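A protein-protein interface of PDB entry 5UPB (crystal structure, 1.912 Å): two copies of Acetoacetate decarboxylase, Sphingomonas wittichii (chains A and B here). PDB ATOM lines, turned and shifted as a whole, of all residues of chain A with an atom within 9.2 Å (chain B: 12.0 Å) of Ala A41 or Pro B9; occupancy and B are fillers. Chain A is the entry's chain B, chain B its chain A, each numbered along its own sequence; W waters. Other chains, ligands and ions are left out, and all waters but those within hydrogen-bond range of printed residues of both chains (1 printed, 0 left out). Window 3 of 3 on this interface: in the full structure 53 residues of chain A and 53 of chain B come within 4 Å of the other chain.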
ATOM      1  N   ASP A  35     -28.828 -28.510  16.367  1.00  0.00           N
ATOM      2  CA  ASP A  35     -28.453 -29.513  15.380  1.00  0.00           C
ATOM      3  C   ASP A  35     -27.680 -30.625  16.077  1.00  0.00           C
ATOM      4  O   ASP A  35     -26.618 -30.362  16.658  1.00  0.00           O
ATOM      5  CB  ASP A  35     -27.613 -28.931  14.244  1.00  0.00           C
ATOM      6  CG  ASP A  35     -27.313 -29.964  13.173  1.00  0.00           C
ATOM      7  OD1 ASP A  35     -28.184 -30.224  12.318  1.00  0.00           O
ATOM      8  OD2 ASP A  35     -26.212 -30.540  13.207  1.00  0.00           O
ATOM      9  N   PRO A  36     -28.170 -31.861  16.065  1.00  0.00           N
ATOM     10  CA  PRO A  36     -27.440 -32.921  16.778  1.00  0.00           C
ATOM     11  C   PRO A  36     -26.004 -33.089  16.310  1.00  0.00           C
ATOM     12  O   PRO A  36     -25.136 -33.436  17.119  1.00  0.00           O
ATOM     13  CB  PRO A  36     -28.274 -34.173  16.473  1.00  0.00           C
ATOM     14  CG  PRO A  36     -29.640 -33.659  16.128  1.00  0.00           C
ATOM     15  CD  PRO A  36     -29.414 -32.347  15.447  1.00  0.00           C
ATOM     16  N   ALA A  37     -25.711 -32.824  15.035  1.00  0.00           N
ATOM     17  CA  ALA A  37     -24.354 -33.039  14.554  1.00  0.00           C
ATOM     18  C   ALA A  37     -23.405 -32.042  15.187  1.00  0.00           C
ATOM     19  O   ALA A  37     -22.260 -32.382  15.509  1.00  0.00           O
ATOM     20  CB  ALA A  37     -24.288 -32.946  13.030  1.00  0.00           C
ATOM     21  N   ARG A  38     -23.847 -30.792  15.349  1.00  0.00           N
ATOM     22  CA  ARG A  38     -22.994 -29.820  16.023  1.00  0.00           C
ATOM     23  C   ARG A  38     -22.749 -30.205  17.469  1.00  0.00           C
ATOM     24  O   ARG A  38     -21.644 -29.986  17.987  1.00  0.00           O
ATOM     25  CB  ARG A  38     -23.597 -28.421  15.942  1.00  0.00           C
ATOM     26  CG  ARG A  38     -23.362 -27.761  14.595  1.00  0.00           C
ATOM     27  CD  ARG A  38     -23.676 -26.276  14.635  1.00  0.00           C
ATOM     28  NE  ARG A  38     -23.531 -25.664  13.317  1.00  0.00           N
ATOM     29  CZ  ARG A  38     -23.941 -24.437  13.014  1.00  0.00           C
ATOM     30  NH1 ARG A  38     -24.530 -23.690  13.941  1.00  0.00           N
ATOM     31  NH2 ARG A  38     -23.765 -23.963  11.783  1.00  0.00           N
ATOM     32  N   LEU A  39     -23.786 -30.667  18.180  1.00  0.00           N
ATOM     33  CA  LEU A  39     -23.545 -31.028  19.573  1.00  0.00           C
ATOM     34  C   LEU A  39     -22.645 -32.253  19.691  1.00  0.00           C
ATOM     35  O   LEU A  39     -21.875 -32.361  20.652  1.00  0.00           O
ATOM     36  CB  LEU A  39     -24.843 -31.230  20.318  1.00  0.00           C
ATOM     37  CG  LEU A  39     -25.797 -30.042  20.236  1.00  0.00           C
ATOM     38  CD1 LEU A  39     -27.070 -30.308  21.017  1.00  0.00           C
ATOM     39  CD2 LEU A  39     -25.149 -28.795  20.724  1.00  0.00           C
ATOM     40  N   GLN A  40     -22.767 -33.205  18.762  1.00  0.00           N
ATOM     41  CA  GLN A  40     -21.952 -34.415  18.829  1.00  0.00           C
ATOM     42  C   GLN A  40     -20.462 -34.073  18.823  1.00  0.00           C
ATOM     43  O   GLN A  40     -19.663 -34.745  19.482  1.00  0.00           O
ATOM     44  CB  GLN A  40     -22.293 -35.333  17.647  1.00  0.00           C
ATOM     45  CG  GLN A  40     -21.522 -36.643  17.644  1.00  0.00           C
ATOM     46  CD  GLN A  40     -21.996 -37.566  18.748  1.00  0.00           C
ATOM     47  OE1 GLN A  40     -23.182 -37.869  18.837  1.00  0.00           O
ATOM     48  NE2 GLN A  40     -21.077 -37.989  19.617  1.00  0.00           N
ATOM     49  N   ALA A  41     -20.074 -33.041  18.062  1.00  0.00           N
ATOM     50  CA  ALA A  41     -18.677 -32.610  18.003  1.00  0.00           C
ATOM     51  C   ALA A  41     -18.148 -32.203  19.377  1.00  0.00           C
ATOM     52  O   ALA A  41     -16.931 -32.169  19.585  1.00  0.00           O
ATOM     53  CB  ALA A  41     -18.531 -31.453  17.016  1.00  0.00           C
ATOM     54  N   LEU A  42     -19.036 -31.784  20.293  1.00  0.00           N
ATOM     55  CA  LEU A  42     -18.641 -31.416  21.651  1.00  0.00           C
ATOM     56  C   LEU A  42     -18.585 -32.591  22.619  1.00  0.00           C
ATOM     57  O   LEU A  42     -18.119 -32.407  23.752  1.00  0.00           O
ATOM     58  CB  LEU A  42     -19.588 -30.342  22.226  1.00  0.00           C
ATOM     59  CG  LEU A  42     -19.632 -28.998  21.500  1.00  0.00           C
ATOM     60  CD1 LEU A  42     -20.644 -28.033  22.084  1.00  0.00           C
ATOM     61  CD2 LEU A  42     -18.231 -28.383  21.572  1.00  0.00           C
ATOM     62  N   LEU A  43     -19.119 -33.762  22.241  1.00  0.00           N
ATOM     63  CA  LEU A  43     -19.180 -34.891  23.159  1.00  0.00           C
ATOM     64  C   LEU A  43     -17.894 -35.709  23.138  1.00  0.00           C
ATOM     65  O   LEU A  43     -17.339 -35.970  22.068  1.00  0.00           O
ATOM     66  CB  LEU A  43     -20.346 -35.822  22.825  1.00  0.00           C
ATOM     67  CG  LEU A  43     -21.715 -35.201  23.002  1.00  0.00           C
ATOM     68  CD1 LEU A  43     -22.873 -36.163  22.539  1.00  0.00           C
ATOM     69  CD2 LEU A  43     -21.912 -34.754  24.469  1.00  0.00           C
ATOM     70  N   PRO A  44     -17.427 -36.162  24.295  1.00  0.00           N
ATOM     71  CA  PRO A  44     -16.298 -37.088  24.305  1.00  0.00           C
ATOM     72  C   PRO A  44     -16.670 -38.457  23.755  1.00  0.00           C
ATOM     73  O   PRO A  44     -17.834 -38.867  23.708  1.00  0.00           O
ATOM     74  CB  PRO A  44     -15.913 -37.146  25.784  1.00  0.00           C
ATOM     75  CG  PRO A  44     -17.134 -36.838  26.510  1.00  0.00           C
ATOM     76  CD  PRO A  44     -17.874 -35.828  25.656  1.00  0.00           C
ATOM     77  N   ALA A  45     -15.643 -39.167  23.316  1.00  0.00           N
ATOM     78  CA  ALA A  45     -15.851 -40.461  22.685  1.00  0.00           C
ATOM     79  C   ALA A  45     -16.632 -41.389  23.611  1.00  0.00           C
ATOM     80  O   ALA A  45     -16.337 -41.489  24.807  1.00  0.00           O
ATOM     81  CB  ALA A  45     -14.507 -41.081  22.319  1.00  0.00           C
ATOM     82  N   LEU A  47     -20.067 -41.154  23.969  1.00  0.00           N
ATOM     83  CA  LEU A  47     -21.379 -40.561  24.173  1.00  0.00           C
ATOM     84  C   LEU A  47     -21.988 -40.212  22.820  1.00  0.00           C
ATOM     85  O   LEU A  47     -21.287 -39.747  21.911  1.00  0.00           O
ATOM     86  CB  LEU A  47     -21.251 -39.310  25.036  1.00  0.00           C
ATOM     87  CG  LEU A  47     -20.641 -39.481  26.444  1.00  0.00           C
ATOM     88  CD1 LEU A  47     -20.674 -38.153  27.215  1.00  0.00           C
ATOM     89  CD2 LEU A  47     -21.336 -40.559  27.257  1.00  0.00           C
ATOM     90  N   LYS A  48     -23.280 -40.492  22.680  1.00  0.00           N
ATOM     91  CA  LYS A  48     -24.042 -40.262  21.452  1.00  0.00           C
ATOM     92  C   LYS A  48     -25.109 -39.229  21.746  1.00  0.00           C
ATOM     93  O   LYS A  48     -25.827 -39.335  22.748  1.00  0.00           O
ATOM     94  CB  LYS A  48     -24.692 -41.538  20.890  1.00  0.00           C
ATOM     95  CG  LYS A  48     -23.717 -42.535  20.244  1.00  0.00           C
ATOM     96  CD  LYS A  48     -22.845 -41.910  19.148  1.00  0.00           C
ATOM     97  CE  LYS A  48     -21.792 -42.886  18.640  1.00  0.00           C
ATOM     98  NZ  LYS A  48     -20.859 -42.253  17.665  1.00  0.00           N
ATOM     99  N   VAL A  49     -25.182 -38.205  20.903  1.00  0.00           N
ATOM    100  CA  VAL A  49     -26.152 -37.156  21.130  1.00  0.00           C
ATOM    101  C   VAL A  49     -27.549 -37.773  21.055  1.00  0.00           C
ATOM    102  O   VAL A  49     -27.779 -38.776  20.365  1.00  0.00           O
ATOM    103  CB  VAL A  49     -25.976 -36.023  20.105  1.00  0.00           C
ATOM    104  CG1 VAL A  49     -26.377 -36.514  18.675  1.00  0.00           C
ATOM    105  CG2 VAL A  49     -26.737 -34.798  20.536  1.00  0.00           C
ATOM    106  N   ILE A  88     -25.769 -31.102  27.253  1.00  0.00           N
ATOM    107  CA  ILE A  88     -26.195 -31.802  26.044  1.00  0.00           C
ATOM    108  C   ILE A  88     -26.811 -33.125  26.448  1.00  0.00           C
ATOM    109  O   ILE A  88     -26.189 -33.912  27.166  1.00  0.00           O
ATOM    110  CB  ILE A  88     -25.008 -32.050  25.096  1.00  0.00           C
ATOM    111  CG1 ILE A  88     -24.351 -30.723  24.702  1.00  0.00           C
ATOM    112  CG2 ILE A  88     -25.451 -32.928  23.880  1.00  0.00           C
ATOM    113  CD1 ILE A  88     -23.024 -30.915  23.964  1.00  0.00           C
ATOM    114  N   PHE A  99     -24.373 -34.400  29.258  1.00  0.00           N
ATOM    115  CA  PHE A  99     -22.961 -34.011  29.316  1.00  0.00           C
ATOM    116  C   PHE A  99     -22.935 -32.505  29.465  1.00  0.00           C
ATOM    117  O   PHE A  99     -23.261 -31.784  28.502  1.00  0.00           O
ATOM    118  CB  PHE A  99     -22.152 -34.424  28.074  1.00  0.00           C
ATOM    119  CG  PHE A  99     -20.712 -33.963  28.121  1.00  0.00           C
ATOM    120  CD1 PHE A  99     -19.823 -34.535  29.013  1.00  0.00           C
ATOM    121  CD2 PHE A  99     -20.254 -32.967  27.282  1.00  0.00           C
ATOM    122  CE1 PHE A  99     -18.488 -34.115  29.071  1.00  0.00           C
ATOM    123  CE2 PHE A  99     -18.924 -32.525  27.345  1.00  0.00           C
ATOM    124  CZ  PHE A  99     -18.044 -33.108  28.224  1.00  0.00           C
ATOM    125  N   ALA A 101     -21.388 -29.648  28.809  1.00  0.00           N
ATOM    126  CA  ALA A 101     -20.225 -29.250  28.010  1.00  0.00           C
ATOM    127  C   ALA A 101     -19.603 -27.956  28.498  1.00  0.00           C
ATOM    128  O   ALA A 101     -18.372 -27.848  28.588  1.00  0.00           O
ATOM    129  CB  ALA A 101     -20.624 -29.118  26.545  1.00  0.00           C
ATOM    130  N   PHE A 102     -20.417 -26.914  28.681  1.00  0.00           N
ATOM    131  CA  PHE A 102     -19.920 -25.607  29.103  1.00  0.00           C
ATOM    132  C   PHE A 102     -20.569 -25.242  30.435  1.00  0.00           C
ATOM    133  O   PHE A 102     -21.798 -25.127  30.526  1.00  0.00           O
ATOM    134  CB  PHE A 102     -20.236 -24.517  28.052  1.00  0.00           C
ATOM    135  CG  PHE A 102     -19.708 -24.790  26.646  1.00  0.00           C
ATOM    136  CD1 PHE A 102     -18.669 -25.669  26.410  1.00  0.00           C
ATOM    137  CD2 PHE A 102     -20.309 -24.185  25.561  1.00  0.00           C
ATOM    138  CE1 PHE A 102     -18.211 -25.905  25.099  1.00  0.00           C
ATOM    139  CE2 PHE A 102     -19.870 -24.419  24.255  1.00  0.00           C
ATOM    140  CZ  PHE A 102     -18.825 -25.276  24.024  1.00  0.00           C
ATOM    141  N   ALA A 228     -17.008 -21.140  22.826  1.00  0.00           N
ATOM    142  CA  ALA A 228     -17.582 -21.731  21.623  1.00  0.00           C
ATOM    143  C   ALA A 228     -19.092 -21.720  21.715  1.00  0.00           C
ATOM    144  O   ALA A 228     -19.764 -22.714  21.441  1.00  0.00           O
ATOM    145  CB  ALA A 228     -17.076 -23.156  21.432  1.00  0.00           C
ATOM    146  N   CYS A 231     -21.787 -22.966  19.111  1.00  0.00           N
ATOM    147  CA  CYS A 231     -22.224 -24.344  18.981  1.00  0.00           C
ATOM    148  C   CYS A 231     -23.675 -24.531  19.385  1.00  0.00           C
ATOM    149  O   CYS A 231     -24.316 -25.482  18.914  1.00  0.00           O
ATOM    150  CB  CYS A 231     -21.346 -25.278  19.829  1.00  0.00           C
ATOM    151  SG  CYS A 231     -19.593 -25.338  19.313  1.00  0.00           S
ATOM    152  N   ALA B   3      -3.955 -29.181  25.633  1.00  0.00           N
ATOM    153  CA  ALA B   3      -5.101 -28.299  25.806  1.00  0.00           C
ATOM    154  C   ALA B   3      -6.114 -28.953  26.773  1.00  0.00           C
ATOM    155  O   ALA B   3      -6.132 -30.170  26.964  1.00  0.00           O
ATOM    156  CB  ALA B   3      -5.742 -27.964  24.439  1.00  0.00           C
ATOM    157  N   THR B   4      -6.933 -28.125  27.393  1.00  0.00           N
ATOM    158  CA  THR B   4      -7.805 -28.486  28.519  1.00  0.00           C
ATOM    159  C   THR B   4      -9.256 -28.222  28.142  1.00  0.00           C
ATOM    160  O   THR B   4      -9.553 -27.740  27.038  1.00  0.00           O
ATOM    161  CB  THR B   4      -7.458 -27.662  29.759  1.00  0.00           C
ATOM    162  OG1 THR B   4      -7.848 -26.294  29.527  1.00  0.00           O
ATOM    163  CG2 THR B   4      -5.963 -27.714  30.063  1.00  0.00           C
ATOM    164  N   HIS B   5     -10.167 -28.527  29.080  1.00  0.00           N
ATOM    165  CA  HIS B   5     -11.539 -28.043  28.953  1.00  0.00           C
ATOM    166  C   HIS B   5     -11.525 -26.543  28.677  1.00  0.00           C
ATOM    167  O   HIS B   5     -10.655 -25.823  29.183  1.00  0.00           O
ATOM    168  CB  HIS B   5     -12.361 -28.248  30.241  1.00  0.00           C
ATOM    169  CG  HIS B   5     -12.390 -29.649  30.771  1.00  0.00           C
ATOM    170  ND1 HIS B   5     -12.895 -30.709  30.054  1.00  0.00           N
ATOM    171  CD2 HIS B   5     -12.021 -30.151  31.979  1.00  0.00           C
ATOM    172  CE1 HIS B   5     -12.821 -31.809  30.785  1.00  0.00           C
ATOM    173  NE2 HIS B   5     -12.295 -31.501  31.959  1.00  0.00           N
ATOM    174  N   PHE B   6     -12.501 -26.048  27.906  1.00  0.00           N
ATOM    175  CA  PHE B   6     -13.485 -26.854  27.144  1.00  0.00           C
ATOM    176  C   PHE B   6     -12.864 -27.426  25.869  1.00  0.00           C
ATOM    177  O   PHE B   6     -12.372 -26.674  25.016  1.00  0.00           O
ATOM    178  CB  PHE B   6     -14.710 -26.012  26.754  1.00  0.00           C
ATOM    179  CG  PHE B   6     -15.380 -25.292  27.914  1.00  0.00           C
ATOM    180  CD1 PHE B   6     -15.412 -25.847  29.180  1.00  0.00           C
ATOM    181  CD2 PHE B   6     -15.972 -24.050  27.714  1.00  0.00           C
ATOM    182  CE1 PHE B   6     -16.011 -25.184  30.242  1.00  0.00           C
ATOM    183  CE2 PHE B   6     -16.584 -23.375  28.769  1.00  0.00           C
ATOM    184  CZ  PHE B   6     -16.602 -23.949  30.042  1.00  0.00           C
ATOM    185  N   LEU B   7     -12.899 -28.745  25.716  1.00  0.00           N
ATOM    186  CA  LEU B   7     -12.345 -29.389  24.524  1.00  0.00           C
ATOM    187  C   LEU B   7     -13.330 -29.306  23.360  1.00  0.00           C
ATOM    188  O   LEU B   7     -14.442 -29.845  23.429  1.00  0.00           O
ATOM    189  CB  LEU B   7     -11.992 -30.845  24.825  1.00  0.00           C
ATOM    190  CG  LEU B   7     -10.887 -31.076  25.851  1.00  0.00           C
ATOM    191  CD1 LEU B   7     -10.791 -32.540  26.204  1.00  0.00           C
ATOM    192  CD2 LEU B   7      -9.548 -30.554  25.289  1.00  0.00           C
ATOM    193  N   THR B   8     -12.922 -28.641  22.292  1.00  0.00           N
ATOM    194  CA  THR B   8     -13.726 -28.529  21.086  1.00  0.00           C
ATOM    195  C   THR B   8     -12.786 -28.741  19.912  1.00  0.00           C
ATOM    196  O   THR B   8     -11.567 -28.578  20.054  1.00  0.00           O
ATOM    197  CB  THR B   8     -14.433 -27.168  20.963  1.00  0.00           C
ATOM    198  OG1 THR B   8     -13.512 -26.174  20.480  1.00  0.00           O
ATOM    199  CG2 THR B   8     -14.973 -26.711  22.300  1.00  0.00           C
ATOM    200  N   PRO B   9     -13.317 -29.114  18.738  1.00  0.00           N
ATOM    201  CA  PRO B   9     -12.410 -29.383  17.602  1.00  0.00           C
ATOM    202  C   PRO B   9     -11.516 -28.194  17.291  1.00  0.00           C
ATOM    203  O   PRO B   9     -10.292 -28.341  17.189  1.00  0.00           O
ATOM    204  CB  PRO B   9     -13.369 -29.721  16.448  1.00  0.00           C
ATOM    205  CG  PRO B   9     -14.743 -29.890  17.071  1.00  0.00           C
ATOM    206  CD  PRO B   9     -14.734 -29.091  18.336  1.00  0.00           C
ATOM    207  N   THR B  10     -12.116 -27.012  17.128  1.00  0.00           N
ATOM    208  CA  THR B  10     -11.380 -25.753  17.067  1.00  0.00           C
ATOM    209  C   THR B  10     -10.289 -25.638  18.131  1.00  0.00           C
ATOM    210  O   THR B  10      -9.141 -25.283  17.836  1.00  0.00           O
ATOM    211  CB  THR B  10     -12.368 -24.599  17.230  1.00  0.00           C
ATOM    212  OG1 THR B  10     -13.442 -24.756  16.299  1.00  0.00           O
ATOM    213  CG2 THR B  10     -11.680 -23.272  16.993  1.00  0.00           C
ATOM    214  N   GLY B  11     -10.642 -25.895  19.385  1.00  0.00           N
ATOM    215  CA  GLY B  11      -9.752 -25.630  20.493  1.00  0.00           C
ATOM    216  C   GLY B  11      -9.774 -24.196  20.986  1.00  0.00           C
ATOM    217  O   GLY B  11      -9.023 -23.866  21.918  1.00  0.00           O
ATOM    218  N   GLN B  12     -10.629 -23.339  20.416  1.00  0.00           N
ATOM    219  CA  GLN B  12     -10.699 -21.942  20.830  1.00  0.00           C
ATOM    220  C   GLN B  12     -11.196 -21.773  22.255  1.00  0.00           C
ATOM    221  O   GLN B  12     -11.073 -20.678  22.815  1.00  0.00           O
ATOM    222  CB  GLN B  12     -11.617 -21.160  19.883  1.00  0.00           C
ATOM    223  CG  GLN B  12     -13.018 -21.758  19.732  1.00  0.00           C
ATOM    224  CD  GLN B  12     -13.968 -20.827  19.022  1.00  0.00           C
ATOM    225  OE1 GLN B  12     -13.574 -19.765  18.543  1.00  0.00           O
ATOM    226  NE2 GLN B  12     -15.234 -21.216  18.955  1.00  0.00           N
ATOM    227  N   ALA B  13     -11.778 -22.810  22.849  1.00  0.00           N
ATOM    228  CA  ALA B  13     -12.415 -22.680  24.146  1.00  0.00           C
ATOM    229  C   ALA B  13     -11.610 -23.326  25.265  1.00  0.00           C
ATOM    230  O   ALA B  13     -12.108 -23.405  26.385  1.00  0.00           O
ATOM    231  CB  ALA B  13     -13.831 -23.274  24.101  1.00  0.00           C
ATOM    232  N   SER B  14     -10.398 -23.815  24.991  1.00  0.00           N
ATOM    233  CA  SER B  14      -9.583 -24.407  26.045  1.00  0.00           C
ATOM    234  C   SER B  14      -9.053 -23.309  26.951  1.00  0.00           C
ATOM    235  O   SER B  14      -8.605 -22.263  26.482  1.00  0.00           O
ATOM    236  CB  SER B  14      -8.401 -25.204  25.464  1.00  0.00           C
ATOM    237  OG  SER B  14      -8.794 -26.435  24.882  1.00  0.00           O
ATOM    238  N   LEU B  15      -9.087 -23.548  28.264  1.00  0.00           N
ATOM    239  CA  LEU B  15      -8.485 -22.593  29.196  1.00  0.00           C
ATOM    240  C   LEU B  15      -7.006 -22.421  28.932  1.00  0.00           C
ATOM    241  O   LEU B  15      -6.467 -21.319  29.060  1.00  0.00           O
ATOM    242  CB  LEU B  15      -8.650 -23.054  30.634  1.00  0.00           C
ATOM    243  CG  LEU B  15      -9.830 -22.659  31.471  1.00  0.00           C
ATOM    244  CD1 LEU B  15      -9.596 -23.254  32.876  1.00  0.00           C
ATOM    245  CD2 LEU B  15     -10.044 -21.172  31.531  1.00  0.00           C
ATOM    246  N   VAL B  16      -6.326 -23.522  28.640  1.00  0.00           N
ATOM    247  CA  VAL B  16      -4.877 -23.574  28.557  1.00  0.00           C
ATOM    248  C   VAL B  16      -4.528 -24.382  27.317  1.00  0.00           C
ATOM    249  O   VAL B  16      -5.236 -25.335  26.974  1.00  0.00           O
ATOM    250  CB  VAL B  16      -4.280 -24.216  29.837  1.00  0.00           C
ATOM    251  CG1 VAL B  16      -2.786 -24.322  29.716  1.00  0.00           C
ATOM    252  CG2 VAL B  16      -4.665 -23.404  31.080  1.00  0.00           C
ATOM    253  N   ASP B  17      -3.451 -23.996  26.637  1.00  0.00           N
ATOM    254  CA  ASP B  17      -2.864 -24.775  25.545  1.00  0.00           C
ATOM    255  C   ASP B  17      -1.449 -25.179  25.948  1.00  0.00           C
ATOM    256  O   ASP B  17      -0.918 -24.713  26.957  1.00  0.00           O
ATOM    257  CB  ASP B  17      -2.863 -23.974  24.233  1.00  0.00           C
ATOM    258  CG  ASP B  17      -2.474 -22.522  24.440  1.00  0.00           C
ATOM    259  OD1 ASP B  17      -1.983 -22.215  25.540  1.00  0.00           O
ATOM    260  OD2 ASP B  17      -2.681 -21.683  23.538  1.00  0.00           O
ATOM    261  N   ASP B  18      -0.830 -26.084  25.192  1.00  0.00           N
ATOM    262  CA  ASP B  18       0.544 -26.472  25.507  1.00  0.00           C
ATOM    263  C   ASP B  18       1.570 -25.671  24.707  1.00  0.00           C
ATOM    264  O   ASP B  18       2.696 -26.134  24.483  1.00  0.00           O
ATOM    265  CB  ASP B  18       0.746 -27.978  25.308  1.00  0.00           C
ATOM    266  CG  ASP B  18       0.316 -28.455  23.952  1.00  0.00           C
ATOM    267  OD1 ASP B  18      -0.560 -27.804  23.346  1.00  0.00           O
ATOM    268  OD2 ASP B  18       0.852 -29.491  23.502  1.00  0.00           O
ATOM    269  N   GLN B  68      -0.189 -17.290  19.869  1.00  0.00           N
ATOM    270  CA  GLN B  68      -1.334 -16.384  19.786  1.00  0.00           C
ATOM    271  C   GLN B  68      -0.836 -15.059  20.339  1.00  0.00           C
ATOM    272  O   GLN B  68      -1.366 -14.510  21.321  1.00  0.00           O
ATOM    273  CB  GLN B  68      -2.554 -16.907  20.542  1.00  0.00           C
ATOM    274  CG  GLN B  68      -3.572 -17.601  19.665  1.00  0.00           C
ATOM    275  CD  GLN B  68      -4.919 -17.723  20.348  1.00  0.00           C
ATOM    276  OE1 GLN B  68      -5.120 -18.590  21.201  1.00  0.00           O
ATOM    277  NE2 GLN B  68      -5.845 -16.838  19.992  1.00  0.00           N
HETATM  278  O   HOH W   1     -16.848 -30.078  24.775  1.00  0.00           O
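Water W1 bridges O of Leu B7 and O of Leu A42.
The backbone carbonyl oxygen (O) of Ala B13 is in hydrogen-bond range of the backbone NH (N) of Phe B6, at 3.1 Å.
OG1 of Thr B8 sits at hydrogen-bond distance from N of Gly B11 (3.1 Å).
The backbone carbonyl oxygen of Phe B6 lies within hydrogen-bond range of the backbone NH of Ser B14, 3.5 Å away.
The side-chain sulfur (SG) of Cys A231 sits at hydrogen-bond distance from the backbone carbonyl oxygen (O) of Ala A228, at 3.4 Å.
Of the printed residues of chain B, Ala A41 touches Pro B9.
Of the printed residues of chain A, Pro B9 touches Ala A41.
No residue of chain B comes within 4 Å of Ala A37.
Of chain B, only Thr B8 comes within 4 Å of Leu A42.
Of chain A, only Leu A42 comes within 4 Å of Thr B8.
Printed residues of chain B within 4 Å of Phe A102: Phe B6.
Of the printed residues of chain B, Ala A101 touches Phe B6 (3.6 Å).
Of the printed residues of chain A, Gln B12 touches Ala A228.
Printed residues of chain A within 4 Å of Phe B6: Ala A101 (3.6 Å) and Phe A102 (3.4 Å).
Pro A36 touches none of the printed residues of chain B.
Val B16 touches none of the printed residues of chain A.
The nearest printed residue of chain B that does not touch Ala A41 is Thr B8 (5.1 Å).
The nearest printed residue of chain A that does not touch Pro B9 is Leu A42 (4.8 Å).
No position is printed for both chains.
Of the 5 pairs that touch across the chains among the printed residues, none has its exchanged pair printed and touching as well.
Among the printed residues, pairs that only touch across the chains: Ala A41 with Pro B9, Leu A42 with Thr B8, Ala A101 with Phe B6, Phe A102 with Phe B6 and Ala A228 with Gln B12.
Along chain B the printed residues that touch a printed residue of chain A span positions 6 to 12.
Of the 20 printed residues of chain A, 5 touch a printed residue of chain B.
Among the printed residues, 5 pairs touch across the chains.
Among the printed residues, no Asp or Glu carboxylate lies within 4 Å of a Lys or Arg side-chain nitrogen of the other chain.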
